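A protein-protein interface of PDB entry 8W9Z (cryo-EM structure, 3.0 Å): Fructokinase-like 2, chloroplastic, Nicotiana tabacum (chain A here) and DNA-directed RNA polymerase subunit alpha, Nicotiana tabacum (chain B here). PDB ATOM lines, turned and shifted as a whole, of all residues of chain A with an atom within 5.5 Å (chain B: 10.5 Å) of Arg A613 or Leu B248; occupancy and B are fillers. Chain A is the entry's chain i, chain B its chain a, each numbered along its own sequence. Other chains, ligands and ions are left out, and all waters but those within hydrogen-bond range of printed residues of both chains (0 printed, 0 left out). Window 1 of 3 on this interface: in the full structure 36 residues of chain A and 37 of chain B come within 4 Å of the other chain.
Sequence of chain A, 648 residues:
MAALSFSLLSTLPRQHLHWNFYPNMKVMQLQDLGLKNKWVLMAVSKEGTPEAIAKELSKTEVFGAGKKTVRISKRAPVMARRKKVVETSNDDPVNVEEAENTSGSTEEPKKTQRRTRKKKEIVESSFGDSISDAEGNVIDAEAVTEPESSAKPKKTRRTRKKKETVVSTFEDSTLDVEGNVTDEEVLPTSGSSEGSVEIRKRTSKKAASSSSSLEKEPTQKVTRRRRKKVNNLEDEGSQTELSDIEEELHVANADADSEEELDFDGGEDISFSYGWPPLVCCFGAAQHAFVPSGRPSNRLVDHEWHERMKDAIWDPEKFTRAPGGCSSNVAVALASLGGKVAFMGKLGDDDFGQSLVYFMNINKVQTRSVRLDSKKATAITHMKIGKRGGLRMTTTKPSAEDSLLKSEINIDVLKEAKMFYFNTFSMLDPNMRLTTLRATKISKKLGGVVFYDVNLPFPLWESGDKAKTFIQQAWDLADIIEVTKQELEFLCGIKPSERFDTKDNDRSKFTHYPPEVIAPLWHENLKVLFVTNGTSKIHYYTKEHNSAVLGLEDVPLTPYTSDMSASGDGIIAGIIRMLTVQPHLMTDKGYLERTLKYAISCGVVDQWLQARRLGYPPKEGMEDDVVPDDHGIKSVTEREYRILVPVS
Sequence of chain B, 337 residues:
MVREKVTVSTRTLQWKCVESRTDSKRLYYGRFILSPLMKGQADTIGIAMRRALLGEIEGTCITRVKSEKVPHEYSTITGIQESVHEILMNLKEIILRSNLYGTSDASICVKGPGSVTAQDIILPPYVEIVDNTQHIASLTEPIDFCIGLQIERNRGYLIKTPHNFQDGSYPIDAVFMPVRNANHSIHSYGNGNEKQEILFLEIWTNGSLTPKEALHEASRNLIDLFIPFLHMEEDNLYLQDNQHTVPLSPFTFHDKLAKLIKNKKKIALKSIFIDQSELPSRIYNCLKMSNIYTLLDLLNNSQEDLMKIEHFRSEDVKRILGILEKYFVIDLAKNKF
OD1 of Asp B224 lies within salt-bridge range of NE of Arg A612, 3.0 Å away. The side-chain carboxylate of Asp A630 lies close to the backbone carbonyl oxygen of Leu B248, at 3.5 Å.
The backbone NH of Ile A633 sits at hydrogen-bond distance from the backbone carbonyl oxygen of Tyr A616. O of Val B246 sits at hydrogen-bond distance from OG of Ser B249, at 2.6 Å.
Among the printed residues, merely in contact across the chains: Trp A608 with Asp B224 (3.1 Å), Asp A630 with Pro B250 (3.2 Å), Ile A633 with Leu B248 (3.4 Å), Leu A609 with His B231 (3.4 Å), Arg A613 with Leu B248 (3.5 Å), Leu A609 with Ile B227 (3.6 Å), Val A627 with Val B246 (3.7 Å), Asp A630 with Ser B249 (3.8 Å), Gly A615 with Leu B248 (3.8 Å), Lys A634 with Leu B248 (3.9 Å) and Val A627 with Ser B249 (3.95 Å).
Arg A613 touches just one residue of chain B: Leu B248 (3.5 Å). Of chain A, only Arg A613 (3.5 Å), Gly A615 (3.8 Å), Asp A630 (3.5 Å), Ile A633 (3.4 Å) and Lys A634 (3.9 Å) come within 4 Å of Leu B248. No residue of chain B comes within 4 Å of Gln A610. No residue of chain B comes within 4 Å of Ala A611. No residue of chain B comes within 4 Å of Leu A614. Gly A615 touches just one residue of chain B: Leu B248. No residue of chain B comes within 4 Å of Gly A632. Of the printed residues of chain A, Pro B250 touches Asp A630. Printed residues of chain B within 4 Å of Val A627: Val B246 and Ser B249. Of the printed residues of chain B, Arg A612 touches Asp B224. Printed residues of chain A within 4 Å of Asp B224: Trp A608 and Arg A612. Of the printed residues of chain A, Ser B249 touches Val A627 and Asp A630. The nearest residue of chain B that does not touch Arg A613 is His B231 (4.7 Å). The nearest residue of chain A that does not touch Leu B248 is Gly A632 (4.2 Å).
Of the 15 printed residues of chain A, 9 touch a printed residue of chain B. Hydrophobic or aromatic side chains of chain A within 4 Å of the printed part of chain B: Trp A608, Leu A609 and Val A627. Printed residues of chain B that touch a printed residue of chain A: Asp B224, Ile B227, His B231, Val B246, Leu B248, Ser B249 and Pro B250. Hydrophobic or aromatic side chains of chain B within 4 Å of the printed part of chain A: Ile B227, His B231, Val B246, Leu B248 and Pro B250. Among the printed residues, Asp or Glu carboxylates within 4 Å of a Lys or Arg side-chain nitrogen of the other chain: Arg A612 with Asp B224 (3.0 Å).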
ATOM      1  N   PHE A 359       8.054  17.293  38.640  1.00  0.00           N
ATOM      2  CA  PHE A 359       7.540  17.240  37.296  1.00  0.00           C
ATOM      3  C   PHE A 359       6.219  16.564  37.310  1.00  0.00           C
ATOM      4  O   PHE A 359       5.275  17.028  36.707  1.00  0.00           O
ATOM      5  CB  PHE A 359       8.478  16.432  36.436  1.00  0.00           C
ATOM      6  CG  PHE A 359       8.107  16.406  34.994  1.00  0.00           C
ATOM      7  CD1 PHE A 359       7.880  17.577  34.306  1.00  0.00           C
ATOM      8  CD2 PHE A 359       8.014  15.208  34.321  1.00  0.00           C
ATOM      9  CE1 PHE A 359       7.543  17.555  32.972  1.00  0.00           C
ATOM     10  CE2 PHE A 359       7.680  15.175  32.988  1.00  0.00           C
ATOM     11  CZ  PHE A 359       7.444  16.351  32.310  1.00  0.00           C
ATOM     12  N   TRP A 608       3.958  15.322  17.749  1.00  0.00           N
ATOM     13  CA  TRP A 608       4.068  16.715  17.318  1.00  0.00           C
ATOM     14  C   TRP A 608       4.571  17.600  18.452  1.00  0.00           C
ATOM     15  O   TRP A 608       5.454  18.447  18.256  1.00  0.00           O
ATOM     16  CB  TRP A 608       2.713  17.224  16.826  1.00  0.00           C
ATOM     17  CG  TRP A 608       2.385  16.919  15.396  1.00  0.00           C
ATOM     18  CD1 TRP A 608       1.879  15.755  14.901  1.00  0.00           C
ATOM     19  CD2 TRP A 608       2.504  17.810  14.281  1.00  0.00           C
ATOM     20  NE1 TRP A 608       1.690  15.859  13.545  1.00  0.00           N
ATOM     21  CE2 TRP A 608       2.065  17.111  13.140  1.00  0.00           C
ATOM     22  CE3 TRP A 608       2.947  19.127  14.137  1.00  0.00           C
ATOM     23  CZ2 TRP A 608       2.056  17.685  11.872  1.00  0.00           C
ATOM     24  CZ3 TRP A 608       2.938  19.694  12.877  1.00  0.00           C
ATOM     25  CH2 TRP A 608       2.496  18.974  11.762  1.00  0.00           C
ATOM     26  N   LEU A 609       4.007  17.424  19.649  1.00  0.00           N
ATOM     27  CA  LEU A 609       4.382  18.262  20.782  1.00  0.00           C
ATOM     28  C   LEU A 609       5.836  18.041  21.177  1.00  0.00           C
ATOM     29  O   LEU A 609       6.548  18.997  21.503  1.00  0.00           O
ATOM     30  CB  LEU A 609       3.458  17.989  21.968  1.00  0.00           C
ATOM     31  CG  LEU A 609       1.990  18.384  21.811  1.00  0.00           C
ATOM     32  CD1 LEU A 609       1.183  17.932  23.016  1.00  0.00           C
ATOM     33  CD2 LEU A 609       1.860  19.879  21.616  1.00  0.00           C
ATOM     34  N   GLN A 610       6.294  16.788  21.161  1.00  0.00           N
ATOM     35  CA  GLN A 610       7.686  16.521  21.505  1.00  0.00           C
ATOM     36  C   GLN A 610       8.636  17.053  20.441  1.00  0.00           C
ATOM     37  O   GLN A 610       9.741  17.499  20.769  1.00  0.00           O
ATOM     38  CB  GLN A 610       7.910  15.024  21.712  1.00  0.00           C
ATOM     39  CG  GLN A 610       9.229  14.698  22.394  1.00  0.00           C
ATOM     40  CD  GLN A 610       9.495  13.210  22.476  1.00  0.00           C
ATOM     41  OE1 GLN A 610       8.888  12.418  21.758  1.00  0.00           O
ATOM     42  NE2 GLN A 610      10.410  12.820  23.358  1.00  0.00           N
ATOM     43  N   ALA A 611       8.230  17.017  19.170  1.00  0.00           N
ATOM     44  CA  ALA A 611       9.079  17.566  18.117  1.00  0.00           C
ATOM     45  C   ALA A 611       9.148  19.084  18.184  1.00  0.00           C
ATOM     46  O   ALA A 611      10.184  19.670  17.852  1.00  0.00           O
ATOM     47  CB  ALA A 611       8.572  17.118  16.747  1.00  0.00           C
ATOM     48  N   ARG A 612       8.064  19.737  18.604  1.00  0.00           N
ATOM     49  CA  ARG A 612       8.075  21.194  18.705  1.00  0.00           C
ATOM     50  C   ARG A 612       8.722  21.680  19.995  1.00  0.00           C
ATOM     51  O   ARG A 612       9.246  22.799  20.035  1.00  0.00           O
ATOM     52  CB  ARG A 612       6.652  21.741  18.590  1.00  0.00           C
ATOM     53  CG  ARG A 612       6.108  21.737  17.171  1.00  0.00           C
ATOM     54  CD  ARG A 612       6.910  22.673  16.283  1.00  0.00           C
ATOM     55  NE  ARG A 612       6.587  22.512  14.869  1.00  0.00           N
ATOM     56  CZ  ARG A 612       7.254  21.720  14.037  1.00  0.00           C
ATOM     57  NH1 ARG A 612       6.891  21.634  12.766  1.00  0.00           N
ATOM     58  NH2 ARG A 612       8.284  21.013  14.477  1.00  0.00           N
ATOM     59  N   ARG A 613       8.698  20.869  21.054  1.00  0.00           N
ATOM     60  CA  ARG A 613       9.335  21.256  22.309  1.00  0.00           C
ATOM     61  C   ARG A 613      10.848  21.083  22.229  1.00  0.00           C
ATOM     62  O   ARG A 613      11.605  22.042  22.404  1.00  0.00           O
ATOM     63  CB  ARG A 613       8.756  20.437  23.466  1.00  0.00           C
ATOM     64  CG  ARG A 613       9.331  20.790  24.825  1.00  0.00           C
ATOM     65  CD  ARG A 613       8.737  19.918  25.916  1.00  0.00           C
ATOM     66  NE  ARG A 613       8.996  18.500  25.682  1.00  0.00           N
ATOM     67  CZ  ARG A 613       8.590  17.524  26.487  1.00  0.00           C
ATOM     68  NH1 ARG A 613       8.871  16.262  26.195  1.00  0.00           N
ATOM     69  NH2 ARG A 613       7.903  17.810  27.585  1.00  0.00           N
ATOM     70  N   LEU A 614      11.304  19.860  21.967  1.00  0.00           N
ATOM     71  CA  LEU A 614      12.721  19.599  21.743  1.00  0.00           C
ATOM     72  C   LEU A 614      13.047  19.929  20.293  1.00  0.00           C
ATOM     73  O   LEU A 614      12.681  19.182  19.381  1.00  0.00           O
ATOM     74  CB  LEU A 614      13.060  18.146  22.061  1.00  0.00           C
ATOM     75  CG  LEU A 614      12.754  17.642  23.470  1.00  0.00           C
ATOM     76  CD1 LEU A 614      13.209  16.201  23.620  1.00  0.00           C
ATOM     77  CD2 LEU A 614      13.414  18.528  24.510  1.00  0.00           C
ATOM     78  N   GLY A 615      13.733  21.047  20.075  1.00  0.00           N
ATOM     79  CA  GLY A 615      14.015  21.497  18.727  1.00  0.00           C
ATOM     80  C   GLY A 615      15.070  20.681  18.013  1.00  0.00           C
ATOM     81  O   GLY A 615      15.395  19.564  18.428  1.00  0.00           O
ATOM     82  N   TYR A 616      15.615  21.230  16.941  1.00  0.00           N
ATOM     83  CA  TYR A 616      16.646  20.561  16.167  1.00  0.00           C
ATOM     84  C   TYR A 616      18.018  20.792  16.788  1.00  0.00           C
ATOM     85  O   TYR A 616      18.255  21.826  17.423  1.00  0.00           O
ATOM     86  CB  TYR A 616      16.653  21.075  14.730  1.00  0.00           C
ATOM     87  CG  TYR A 616      15.459  20.656  13.903  1.00  0.00           C
ATOM     88  CD1 TYR A 616      14.267  21.365  13.959  1.00  0.00           C
ATOM     89  CD2 TYR A 616      15.530  19.562  13.052  1.00  0.00           C
ATOM     90  CE1 TYR A 616      13.178  20.989  13.200  1.00  0.00           C
ATOM     91  CE2 TYR A 616      14.446  19.181  12.288  1.00  0.00           C
ATOM     92  CZ  TYR A 616      13.273  19.899  12.366  1.00  0.00           C
ATOM     93  OH  TYR A 616      12.189  19.521  11.609  1.00  0.00           O
ATOM     94  N   VAL A 627      23.080  26.124  26.160  1.00  0.00           N
ATOM     95  CA  VAL A 627      22.325  25.717  27.351  1.00  0.00           C
ATOM     96  C   VAL A 627      23.234  24.890  28.251  1.00  0.00           C
ATOM     97  O   VAL A 627      24.009  24.060  27.741  1.00  0.00           O
ATOM     98  CB  VAL A 627      21.078  24.928  26.940  1.00  0.00           C
ATOM     99  CG1 VAL A 627      20.250  24.532  28.154  1.00  0.00           C
ATOM    100  CG2 VAL A 627      20.240  25.735  25.957  1.00  0.00           C
ATOM    101  N   ASP A 630      22.502  21.107  27.216  1.00  0.00           N
ATOM    102  CA  ASP A 630      22.398  20.644  25.836  1.00  0.00           C
ATOM    103  C   ASP A 630      22.525  21.850  24.912  1.00  0.00           C
ATOM    104  O   ASP A 630      22.939  22.936  25.332  1.00  0.00           O
ATOM    105  CB  ASP A 630      21.087  19.885  25.608  1.00  0.00           C
ATOM    106  CG  ASP A 630      19.868  20.773  25.747  1.00  0.00           C
ATOM    107  OD1 ASP A 630      19.864  21.641  26.645  1.00  0.00           O
ATOM    108  OD2 ASP A 630      18.916  20.606  24.956  1.00  0.00           O
ATOM    109  N   GLY A 632      20.244  23.333  21.374  1.00  0.00           N
ATOM    110  CA  GLY A 632      19.176  23.101  20.422  1.00  0.00           C
ATOM    111  C   GLY A 632      18.641  24.357  19.767  1.00  0.00           C
ATOM    112  O   GLY A 632      18.563  25.414  20.401  1.00  0.00           O
ATOM    113  N   ILE A 633      18.267  24.253  18.493  1.00  0.00           N
ATOM    114  CA  ILE A 633      17.721  25.367  17.734  1.00  0.00           C
ATOM    115  C   ILE A 633      16.310  25.006  17.280  1.00  0.00           C
ATOM    116  O   ILE A 633      15.868  23.862  17.396  1.00  0.00           O
ATOM    117  CB  ILE A 633      18.604  25.742  16.530  1.00  0.00           C
ATOM    118  CG1 ILE A 633      18.744  24.548  15.585  1.00  0.00           C
ATOM    119  CG2 ILE A 633      19.969  26.221  16.996  1.00  0.00           C
ATOM    120  CD1 ILE A 633      19.621  24.818  14.383  1.00  0.00           C
ATOM    121  N   LYS A 634      15.605  26.005  16.755  1.00  0.00           N
ATOM    122  CA  LYS A 634      14.229  25.829  16.312  1.00  0.00           C
ATOM    123  C   LYS A 634      14.208  25.205  14.917  1.00  0.00           C
ATOM    124  O   LYS A 634      15.228  24.752  14.393  1.00  0.00           O
ATOM    125  CB  LYS A 634      13.489  27.163  16.347  1.00  0.00           C
ATOM    126  CG  LYS A 634      13.420  27.803  17.721  1.00  0.00           C
ATOM    127  CD  LYS A 634      12.724  29.151  17.664  1.00  0.00           C
ATOM    128  CE  LYS A 634      13.458  30.110  16.742  1.00  0.00           C
ATOM    129  NZ  LYS A 634      12.785  31.435  16.667  1.00  0.00           N
ATOM    130  N   ASP B 224       0.270  23.175  12.980  1.00  0.00           N
ATOM    131  CA  ASP B 224       1.276  23.891  13.758  1.00  0.00           C
ATOM    132  C   ASP B 224       0.683  25.096  14.475  1.00  0.00           C
ATOM    133  O   ASP B 224       1.140  25.452  15.567  1.00  0.00           O
ATOM    134  CB  ASP B 224       2.430  24.327  12.857  1.00  0.00           C
ATOM    135  CG  ASP B 224       3.455  23.232  12.656  1.00  0.00           C
ATOM    136  OD1 ASP B 224       3.811  22.564  13.649  1.00  0.00           O
ATOM    137  OD2 ASP B 224       3.905  23.038  11.508  1.00  0.00           O
ATOM    138  N   ILE B 227      -1.377  23.576  17.467  1.00  0.00           N
ATOM    139  CA  ILE B 227      -0.630  22.803  18.465  1.00  0.00           C
ATOM    140  C   ILE B 227      -0.390  23.569  19.763  1.00  0.00           C
ATOM    141  O   ILE B 227      -0.622  22.997  20.840  1.00  0.00           O
ATOM    142  CB  ILE B 227       0.674  22.270  17.845  1.00  0.00           C
ATOM    143  CG1 ILE B 227       0.443  20.898  17.215  1.00  0.00           C
ATOM    144  CG2 ILE B 227       1.787  22.205  18.878  1.00  0.00           C
ATOM    145  CD1 ILE B 227      -0.022  19.848  18.194  1.00  0.00           C
ATOM    146  N   PRO B 228       0.070  24.830  19.751  1.00  0.00           N
ATOM    147  CA  PRO B 228       0.518  25.452  21.012  1.00  0.00           C
ATOM    148  C   PRO B 228      -0.537  25.519  22.106  1.00  0.00           C
ATOM    149  O   PRO B 228      -0.172  25.696  23.274  1.00  0.00           O
ATOM    150  CB  PRO B 228       0.955  26.858  20.576  1.00  0.00           C
ATOM    151  CG  PRO B 228       0.279  27.087  19.279  1.00  0.00           C
ATOM    152  CD  PRO B 228       0.264  25.752  18.619  1.00  0.00           C
ATOM    153  N   LEU B 230      -2.104  23.098  23.252  1.00  0.00           N
ATOM    154  CA  LEU B 230      -1.992  21.861  24.013  1.00  0.00           C
ATOM    155  C   LEU B 230      -0.713  21.779  24.837  1.00  0.00           C
ATOM    156  O   LEU B 230      -0.520  20.794  25.555  1.00  0.00           O
ATOM    157  CB  LEU B 230      -2.079  20.658  23.072  1.00  0.00           C
ATOM    158  CG  LEU B 230      -3.378  20.553  22.274  1.00  0.00           C
ATOM    159  CD1 LEU B 230      -3.373  19.320  21.392  1.00  0.00           C
ATOM    160  CD2 LEU B 230      -4.574  20.537  23.206  1.00  0.00           C
ATOM    161  N   HIS B 231       0.161  22.779  24.751  1.00  0.00           N
ATOM    162  CA  HIS B 231       1.368  22.791  25.561  1.00  0.00           C
ATOM    163  C   HIS B 231       1.034  23.116  27.017  1.00  0.00           C
ATOM    164  O   HIS B 231      -0.111  23.403  27.377  1.00  0.00           O
ATOM    165  CB  HIS B 231       2.373  23.806  25.014  1.00  0.00           C
ATOM    166  CG  HIS B 231       3.209  23.283  23.890  1.00  0.00           C
ATOM    167  ND1 HIS B 231       3.695  24.092  22.885  1.00  0.00           N
ATOM    168  CD2 HIS B 231       3.656  22.035  23.618  1.00  0.00           C
ATOM    169  CE1 HIS B 231       4.399  23.363  22.038  1.00  0.00           C
ATOM    170  NE2 HIS B 231       4.392  22.111  22.459  1.00  0.00           N
ATOM    171  N   MET B 232       2.061  23.064  27.860  1.00  0.00           N
ATOM    172  CA  MET B 232       1.891  23.403  29.265  1.00  0.00           C
ATOM    173  C   MET B 232       1.695  24.904  29.425  1.00  0.00           C
ATOM    174  O   MET B 232       2.359  25.708  28.766  1.00  0.00           O
ATOM    175  CB  MET B 232       3.100  22.936  30.075  1.00  0.00           C
ATOM    176  CG  MET B 232       2.964  23.138  31.575  1.00  0.00           C
ATOM    177  SD  MET B 232       4.373  22.491  32.496  1.00  0.00           S
ATOM    178  CE  MET B 232       5.707  23.458  31.793  1.00  0.00           C
ATOM    179  N   THR B 245      15.245  27.394  32.699  1.00  0.00           N
ATOM    180  CA  THR B 245      14.192  28.304  32.264  1.00  0.00           C
ATOM    181  C   THR B 245      14.289  28.577  30.767  1.00  0.00           C
ATOM    182  O   THR B 245      13.362  29.116  30.164  1.00  0.00           O
ATOM    183  CB  THR B 245      14.249  29.640  33.029  1.00  0.00           C
ATOM    184  OG1 THR B 245      13.214  30.510  32.554  1.00  0.00           O
ATOM    185  CG2 THR B 245      15.601  30.311  32.831  1.00  0.00           C
ATOM    186  N   VAL B 246      15.414  28.203  30.175  1.00  0.00           N
ATOM    187  CA  VAL B 246      15.622  28.405  28.740  1.00  0.00           C
ATOM    188  C   VAL B 246      14.806  27.366  27.974  1.00  0.00           C
ATOM    189  O   VAL B 246      14.864  26.172  28.311  1.00  0.00           O
ATOM    190  CB  VAL B 246      17.106  28.312  28.392  1.00  0.00           C
ATOM    191  CG1 VAL B 246      17.749  27.119  29.087  1.00  0.00           C
ATOM    192  CG2 VAL B 246      17.299  28.227  26.884  1.00  0.00           C
ATOM    193  N   PRO B 247      14.031  27.770  26.969  1.00  0.00           N
ATOM    194  CA  PRO B 247      13.233  26.801  26.211  1.00  0.00           C
ATOM    195  C   PRO B 247      14.116  25.861  25.402  1.00  0.00           C
ATOM    196  O   PRO B 247      15.332  26.032  25.292  1.00  0.00           O
ATOM    197  CB  PRO B 247      12.371  27.680  25.298  1.00  0.00           C
ATOM    198  CG  PRO B 247      12.392  29.037  25.935  1.00  0.00           C
ATOM    199  CD  PRO B 247      13.741  29.156  26.571  1.00  0.00           C
ATOM    200  N   LEU B 248      13.465  24.845  24.830  1.00  0.00           N
ATOM    201  CA  LEU B 248      14.131  23.837  24.002  1.00  0.00           C
ATOM    202  C   LEU B 248      15.224  23.110  24.784  1.00  0.00           C
ATOM    203  O   LEU B 248      16.299  22.815  24.258  1.00  0.00           O
ATOM    204  CB  LEU B 248      14.697  24.449  22.716  1.00  0.00           C
ATOM    205  CG  LEU B 248      13.713  24.859  21.614  1.00  0.00           C
ATOM    206  CD1 LEU B 248      13.012  26.170  21.940  1.00  0.00           C
ATOM    207  CD2 LEU B 248      14.425  24.949  20.273  1.00  0.00           C
ATOM    208  N   SER B 249      14.946  22.819  26.054  1.00  0.00           N
ATOM    209  CA  SER B 249      15.878  22.112  26.917  1.00  0.00           C
ATOM    210  C   SER B 249      15.119  21.044  27.694  1.00  0.00           C
ATOM    211  O   SER B 249      14.083  21.348  28.313  1.00  0.00           O
ATOM    212  CB  SER B 249      16.584  23.077  27.879  1.00  0.00           C
ATOM    213  OG  SER B 249      15.650  23.742  28.709  1.00  0.00           O
ATOM    214  N   PRO B 250      15.587  19.793  27.692  1.00  0.00           N
ATOM    215  CA  PRO B 250      14.878  18.747  28.445  1.00  0.00           C
ATOM    216  C   PRO B 250      14.987  18.902  29.951  1.00  0.00           C
ATOM    217  O   PRO B 250      14.177  18.310  30.676  1.00  0.00           O
ATOM    218  CB  PRO B 250      15.551  17.454  27.967  1.00  0.00           C
ATOM    219  CG  PRO B 250      16.914  17.883  27.541  1.00  0.00           C
ATOM    220  CD  PRO B 250      16.754  19.263  26.967  1.00  0.00           C
ATOM    221  N   PHE B 251      15.954  19.672  30.446  1.00  0.00           N
ATOM    222  CA  PHE B 251      16.133  19.903  31.878  1.00  0.00           C
ATOM    223  C   PHE B 251      15.565  21.248  32.312  1.00  0.00           C
ATOM    224  O   PHE B 251      16.116  21.908  33.197  1.00  0.00           O
ATOM    225  CB  PHE B 251      17.608  19.803  32.253  1.00  0.00           C
ATOM    226  CG  PHE B 251      18.177  18.422  32.108  1.00  0.00           C
ATOM    227  CD1 PHE B 251      18.003  17.480  33.108  1.00  0.00           C
ATOM    228  CD2 PHE B 251      18.892  18.067  30.978  1.00  0.00           C
ATOM    229  CE1 PHE B 251      18.527  16.209  32.981  1.00  0.00           C
ATOM    230  CE2 PHE B 251      19.418  16.798  30.845  1.00  0.00           C
ATOM    231  CZ  PHE B 251      19.236  15.868  31.848  1.00  0.00           C
ATOM    232  N   THR B 252      14.459  21.678  31.700  1.00  0.00           N
ATOM    233  CA  THR B 252      13.863  22.960  32.057  1.00  0.00           C
ATOM    234  C   THR B 252      13.193  22.934  33.425  1.00  0.00           C
ATOM    235  O   THR B 252      12.840  23.997  33.945  1.00  0.00           O
ATOM    236  CB  THR B 252      12.847  23.385  30.994  1.00  0.00           C
ATOM    237  OG1 THR B 252      12.279  24.651  31.354  1.00  0.00           O
ATOM    238  CG2 THR B 252      11.736  22.352  30.878  1.00  0.00           C
ATOM    239  N   PHE B 253      13.008  21.754  34.016  1.00  0.00           N
ATOM    240  CA  PHE B 253      12.387  21.638  35.329  1.00  0.00           C
ATOM    241  C   PHE B 253      13.393  21.459  36.457  1.00  0.00           C
ATOM    242  O   PHE B 253      13.092  21.821  37.601  1.00  0.00           O
ATOM    243  CB  PHE B 253      11.396  20.466  35.350  1.00  0.00           C
ATOM    244  CG  PHE B 253      12.033  19.123  35.124  1.00  0.00           C
ATOM    245  CD1 PHE B 253      12.264  18.657  33.841  1.00  0.00           C
ATOM    246  CD2 PHE B 253      12.387  18.320  36.195  1.00  0.00           C
ATOM    247  CE1 PHE B 253      12.845  17.420  33.631  1.00  0.00           C
ATOM    248  CE2 PHE B 253      12.968  17.083  35.992  1.00  0.00           C
ATOM    249  CZ  PHE B 253      13.197  16.633  34.708  1.00  0.00           C
ATOM    250  N   ASP B 255      16.740  22.795  36.840  1.00  0.00           N
ATOM    251  CA  ASP B 255      17.320  24.068  37.254  1.00  0.00           C
ATOM    252  C   ASP B 255      16.254  25.039  37.741  1.00  0.00           C
ATOM    253  O   ASP B 255      16.507  25.832  38.656  1.00  0.00           O
ATOM    254  CB  ASP B 255      18.116  24.681  36.102  1.00  0.00           C
ATOM    255  CG  ASP B 255      17.304  24.793  34.825  1.00  0.00           C
ATOM    256  OD1 ASP B 255      16.148  24.319  34.805  1.00  0.00           O
ATOM    257  OD2 ASP B 255      17.824  25.355  33.837  1.00  0.00           O
